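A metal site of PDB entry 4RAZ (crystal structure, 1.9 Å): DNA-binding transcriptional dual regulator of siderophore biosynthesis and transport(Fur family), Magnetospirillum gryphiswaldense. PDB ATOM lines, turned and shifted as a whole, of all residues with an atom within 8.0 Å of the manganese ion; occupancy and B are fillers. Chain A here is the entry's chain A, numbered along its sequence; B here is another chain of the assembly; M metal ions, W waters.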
ATOM      1  N   HIS A  89      15.001  18.388 -34.924  1.00  0.00           N
ATOM      2  CA  HIS A  89      13.799  18.303 -34.092  1.00  0.00           C
ATOM      3  C   HIS A  89      13.131  19.660 -33.868  1.00  0.00           C
ATOM      4  O   HIS A  89      13.826  20.664 -33.670  1.00  0.00           O
ATOM      5  CB  HIS A  89      14.112  17.623 -32.765  1.00  0.00           C
ATOM      6  CG  HIS A  89      12.956  17.656 -31.800  1.00  0.00           C
ATOM      7  ND1 HIS A  89      11.855  16.913 -31.979  1.00  0.00           N
ATOM      8  CD2 HIS A  89      12.726  18.440 -30.664  1.00  0.00           C
ATOM      9  CE1 HIS A  89      10.970  17.167 -30.990  1.00  0.00           C
ATOM     10  NE2 HIS A  89      11.512  18.105 -30.188  1.00  0.00           N
ATOM     11  N   HIS A  90      11.799  19.702 -33.922  1.00  0.00           N
ATOM     12  CA  HIS A  90      11.025  20.877 -33.509  1.00  0.00           C
ATOM     13  C   HIS A  90       9.664  20.451 -32.980  1.00  0.00           C
ATOM     14  O   HIS A  90       9.229  19.311 -33.205  1.00  0.00           O
ATOM     15  CB  HIS A  90      10.875  21.897 -34.656  1.00  0.00           C
ATOM     16  CG  HIS A  90      10.166  21.337 -35.877  1.00  0.00           C
ATOM     17  ND1 HIS A  90      10.838  20.755 -36.888  1.00  0.00           N
ATOM     18  CD2 HIS A  90       8.801  21.239 -36.185  1.00  0.00           C
ATOM     19  CE1 HIS A  90       9.965  20.298 -37.811  1.00  0.00           C
ATOM     20  NE2 HIS A  90       8.716  20.601 -37.391  1.00  0.00           N
ATOM     21  N   ASP A  91       9.013  21.359 -32.272  1.00  0.00           N
ATOM     22  CA  ASP A  91       7.661  21.123 -31.772  1.00  0.00           C
ATOM     23  C   ASP A  91       6.752  22.092 -32.474  1.00  0.00           C
ATOM     24  O   ASP A  91       7.214  22.858 -33.335  1.00  0.00           O
ATOM     25  CB  ASP A  91       7.641  21.279 -30.240  1.00  0.00           C
ATOM     26  CG  ASP A  91       8.688  20.421 -29.595  1.00  0.00           C
ATOM     27  OD1 ASP A  91       8.503  19.180 -29.556  1.00  0.00           O
ATOM     28  OD2 ASP A  91       9.726  20.949 -29.136  1.00  0.00           O
ATOM     29  N   HIS A  92       5.458  22.044 -32.167  1.00  0.00           N
ATOM     30  CA  HIS A  92       4.473  22.858 -32.881  1.00  0.00           C
ATOM     31  C   HIS A  92       3.537  23.615 -31.980  1.00  0.00           C
ATOM     32  O   HIS A  92       3.051  23.099 -30.971  1.00  0.00           O
ATOM     33  CB  HIS A  92       3.654  21.977 -33.820  1.00  0.00           C
ATOM     34  CG  HIS A  92       4.503  21.256 -34.838  1.00  0.00           C
ATOM     35  ND1 HIS A  92       5.124  20.092 -34.565  1.00  0.00           N
ATOM     36  CD2 HIS A  92       4.890  21.620 -36.138  1.00  0.00           C
ATOM     37  CE1 HIS A  92       5.850  19.698 -35.645  1.00  0.00           C
ATOM     38  NE2 HIS A  92       5.713  20.635 -36.599  1.00  0.00           N
ATOM     39  N   PHE A 104       8.588  25.525 -33.506  1.00  0.00           N
ATOM     40  CA  PHE A 104       9.534  26.117 -32.561  1.00  0.00           C
ATOM     41  C   PHE A 104      10.475  25.084 -31.958  1.00  0.00           C
ATOM     42  O   PHE A 104      10.195  23.875 -31.987  1.00  0.00           O
ATOM     43  CB  PHE A 104       8.782  26.887 -31.421  1.00  0.00           C
ATOM     44  CG  PHE A 104       8.080  25.983 -30.440  1.00  0.00           C
ATOM     45  CD1 PHE A 104       8.745  25.463 -29.327  1.00  0.00           C
ATOM     46  CD2 PHE A 104       6.723  25.662 -30.615  1.00  0.00           C
ATOM     47  CE1 PHE A 104       8.088  24.640 -28.432  1.00  0.00           C
ATOM     48  CE2 PHE A 104       6.057  24.848 -29.705  1.00  0.00           C
ATOM     49  CZ  PHE A 104       6.743  24.343 -28.615  1.00  0.00           C
ATOM     50  N   THR A 105      11.577  25.557 -31.396  1.00  0.00           N
ATOM     51  CA  THR A 105      12.442  24.718 -30.590  1.00  0.00           C
ATOM     52  C   THR A 105      12.634  25.361 -29.255  1.00  0.00           C
ATOM     53  O   THR A 105      12.500  26.578 -29.141  1.00  0.00           O
ATOM     54  CB  THR A 105      13.836  24.534 -31.230  1.00  0.00           C
ATOM     55  OG1 THR A 105      14.452  25.815 -31.335  1.00  0.00           O
ATOM     56  CG2 THR A 105      13.693  23.926 -32.610  1.00  0.00           C
ATOM     57  N   SER A 106      12.903  24.561 -28.236  1.00  0.00           N
ATOM     58  CA  SER A 106      13.294  25.034 -26.927  1.00  0.00           C
ATOM     59  C   SER A 106      14.245  24.047 -26.270  1.00  0.00           C
ATOM     60  O   SER A 106      13.801  23.049 -25.670  1.00  0.00           O
ATOM     61  CB  SER A 106      12.065  25.259 -26.036  1.00  0.00           C
ATOM     62  OG  SER A 106      12.470  25.473 -24.697  1.00  0.00           O
ATOM     63  N   PRO A 107      15.557  24.297 -26.406  1.00  0.00           N
ATOM     64  CA  PRO A 107      16.562  23.485 -25.733  1.00  0.00           C
ATOM     65  C   PRO A 107      16.313  23.385 -24.222  1.00  0.00           C
ATOM     66  O   PRO A 107      16.555  22.329 -23.627  1.00  0.00           O
ATOM     67  CB  PRO A 107      17.876  24.228 -26.014  1.00  0.00           C
ATOM     68  CG  PRO A 107      17.639  24.943 -27.296  1.00  0.00           C
ATOM     69  CD  PRO A 107      16.165  25.257 -27.355  1.00  0.00           C
ATOM     70  N   ILE A 109      13.390  23.380 -22.696  1.00  0.00           N
ATOM     71  CA  ILE A 109      12.325  22.387 -22.483  1.00  0.00           C
ATOM     72  C   ILE A 109      12.869  20.973 -22.739  1.00  0.00           C
ATOM     73  O   ILE A 109      12.571  20.035 -22.010  1.00  0.00           O
ATOM     74  CB  ILE A 109      11.065  22.646 -23.348  1.00  0.00           C
ATOM     75  CG1 ILE A 109      10.357  23.915 -22.828  1.00  0.00           C
ATOM     76  CG2 ILE A 109      10.088  21.456 -23.280  1.00  0.00           C
ATOM     77  CD1 ILE A 109       9.089  24.300 -23.593  1.00  0.00           C
ATOM     78  N   GLU A 110      13.702  20.837 -23.773  1.00  0.00           N
ATOM     79  CA  GLU A 110      14.239  19.518 -24.125  1.00  0.00           C
ATOM     80  C   GLU A 110      15.058  18.953 -22.971  1.00  0.00           C
ATOM     81  O   GLU A 110      14.909  17.779 -22.622  1.00  0.00           O
ATOM     82  CB  GLU A 110      15.068  19.562 -25.418  1.00  0.00           C
ATOM     83  CG  GLU A 110      14.288  20.061 -26.641  1.00  0.00           C
ATOM     84  CD  GLU A 110      13.137  19.145 -27.075  1.00  0.00           C
ATOM     85  OE1 GLU A 110      12.195  19.640 -27.747  1.00  0.00           O
ATOM     86  OE2 GLU A 110      13.161  17.931 -26.791  1.00  0.00           O
ATOM     87  N   GLN A 113      12.701  17.814 -20.027  1.00  0.00           N
ATOM     88  CA  GLN A 113      12.074  16.522 -20.377  1.00  0.00           C
ATOM     89  C   GLN A 113      13.010  15.356 -20.067  1.00  0.00           C
ATOM     90  O   GLN A 113      12.595  14.353 -19.488  1.00  0.00           O
ATOM     91  CB  GLN A 113      11.680  16.465 -21.877  1.00  0.00           C
ATOM     92  CG  GLN A 113      10.550  17.421 -22.217  1.00  0.00           C
ATOM     93  CD  GLN A 113      10.267  17.565 -23.712  1.00  0.00           C
ATOM     94  OE1 GLN A 113       9.288  18.201 -24.080  1.00  0.00           O
ATOM     95  NE2 GLN A 113      11.112  16.963 -24.572  1.00  0.00           N
ATOM     96  N   GLY A 126      11.114   9.250 -27.216  1.00  0.00           N
ATOM     97  CA  GLY A 126      10.274  10.090 -28.085  1.00  0.00           C
ATOM     98  C   GLY A 126       9.402  11.003 -27.216  1.00  0.00           C
ATOM     99  O   GLY A 126       9.350  10.825 -26.001  1.00  0.00           O
ATOM    100  N   HIS A 127       8.766  11.989 -27.836  1.00  0.00           N
ATOM    101  CA  HIS A 127       7.807  12.793 -27.101  1.00  0.00           C
ATOM    102  C   HIS A 127       6.975  13.534 -28.086  1.00  0.00           C
ATOM    103  O   HIS A 127       7.328  13.590 -29.277  1.00  0.00           O
ATOM    104  CB  HIS A 127       8.535  13.765 -26.172  1.00  0.00           C
ATOM    105  CG  HIS A 127       9.315  14.835 -26.905  1.00  0.00           C
ATOM    106  ND1 HIS A 127      10.557  14.624 -27.355  1.00  0.00           N
ATOM    107  CD2 HIS A 127       8.953  16.137 -27.275  1.00  0.00           C
ATOM    108  CE1 HIS A 127      11.001  15.739 -27.972  1.00  0.00           C
ATOM    109  NE2 HIS A 127      10.027  16.675 -27.916  1.00  0.00           N
ATOM    110  N   ARG A 128       5.885  14.119 -27.596  1.00  0.00           N
ATOM    111  CA  ARG A 128       4.992  14.928 -28.411  1.00  0.00           C
ATOM    112  C   ARG A 128       4.709  16.176 -27.570  1.00  0.00           C
ATOM    113  O   ARG A 128       4.244  16.050 -26.435  1.00  0.00           O
ATOM    114  CB  ARG A 128       3.703  14.157 -28.659  1.00  0.00           C
ATOM    115  CG  ARG A 128       2.602  14.984 -29.301  1.00  0.00           C
ATOM    116  CD  ARG A 128       1.235  14.331 -29.100  1.00  0.00           C
ATOM    117  NE  ARG A 128       1.118  13.092 -29.862  1.00  0.00           N
ATOM    118  CZ  ARG A 128       0.635  13.006 -31.100  1.00  0.00           C
ATOM    119  NH1 ARG A 128       0.187  14.086 -31.754  1.00  0.00           N
ATOM    120  NH2 ARG A 128       0.577  11.830 -31.704  1.00  0.00           N
ATOM    121  N   LEU A 129       5.024  17.354 -28.113  1.00  0.00           N
ATOM    122  CA  LEU A 129       4.689  18.643 -27.449  1.00  0.00           C
ATOM    123  C   LEU A 129       3.948  19.494 -28.488  1.00  0.00           C
ATOM    124  O   LEU A 129       4.532  19.857 -29.522  1.00  0.00           O
ATOM    125  CB  LEU A 129       5.943  19.389 -26.978  1.00  0.00           C
ATOM    126  CG  LEU A 129       5.615  20.801 -26.432  1.00  0.00           C
ATOM    127  CD1 LEU A 129       4.626  20.710 -25.246  1.00  0.00           C
ATOM    128  CD2 LEU A 129       6.873  21.570 -26.035  1.00  0.00           C
ATOM    129  N   GLU A 130       2.664  19.754 -28.227  1.00  0.00           N
ATOM    130  CA  GLU A 130       1.867  20.627 -29.056  1.00  0.00           C
ATOM    131  C   GLU A 130       1.277  21.720 -28.170  1.00  0.00           C
ATOM    132  O   GLU A 130       0.741  21.427 -27.101  1.00  0.00           O
ATOM    133  CB  GLU A 130       0.727  19.843 -29.699  1.00  0.00           C
ATOM    134  CG  GLU A 130       1.280  18.767 -30.665  1.00  0.00           C
ATOM    135  CD  GLU A 130       0.255  17.700 -30.996  1.00  0.00           C
ATOM    136  OE1 GLU A 130       0.616  16.684 -31.640  1.00  0.00           O
ATOM    137  OE2 GLU A 130      -0.933  17.866 -30.631  1.00  0.00           O
ATOM    138  N   LEU B 129       1.487  17.491 -23.695  1.00  0.00           N
ATOM    139  CA  LEU B 129       2.869  17.077 -23.501  1.00  0.00           C
ATOM    140  C   LEU B 129       2.865  15.618 -23.078  1.00  0.00           C
ATOM    141  O   LEU B 129       2.306  15.266 -22.025  1.00  0.00           O
ATOM    142  CB  LEU B 129       3.599  17.934 -22.466  1.00  0.00           C
ATOM    143  CG  LEU B 129       5.033  17.441 -22.211  1.00  0.00           C
ATOM    144  CD1 LEU B 129       5.879  17.467 -23.484  1.00  0.00           C
ATOM    145  CD2 LEU B 129       5.705  18.242 -21.086  1.00  0.00           C
ATOM    146  N   LEU B 131       5.570  12.283 -22.877  1.00  0.00           N
ATOM    147  CA  LEU B 131       6.935  11.777 -22.967  1.00  0.00           C
ATOM    148  C   LEU B 131       6.857  10.248 -23.098  1.00  0.00           C
ATOM    149  O   LEU B 131       6.102   9.596 -22.379  1.00  0.00           O
ATOM    150  CB  LEU B 131       7.704  12.116 -21.702  1.00  0.00           C
ATOM    151  CG  LEU B 131       7.862  13.593 -21.334  1.00  0.00           C
ATOM    152  CD1 LEU B 131       8.826  13.704 -20.153  1.00  0.00           C
ATOM    153  CD2 LEU B 131       8.358  14.373 -22.552  1.00  0.00           C
HETATM  154 MN    MN M   1      10.464  18.794 -28.433  1.00  0.00          MN
HETATM  155  O   HOH W   1       9.561  19.392 -26.436  1.00  0.00           O
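The side-chain amide nitrogen of Gln 113 sits at hydrogen-bond distance from the side-chain carboxylate of Glu 110, 3.2 Å away.
The backbone NH (N) of Asp 91 lies within hydrogen-bond range of the backbone carbonyl oxygen (O) of Phe 104 (2.8 Å).
Within 4 Å of the manganese ion: His 89, Asp 91, Glu 110 and His 127.
The nearest printed residue that does not touch the manganese ion is Gln 113 (4.3 Å).
The manganese ion is bound by the side-chain carboxylate (OE1) of Glu 110, a ring nitrogen (NE2) of His 89, a ring nitrogen (NE2) of His 127, water W1, the side-chain carboxylate (OD1) of Asp 91 and the side-chain carboxylate (OD2) of Asp 91.
The manganese ion has six donor atoms within binding distance.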
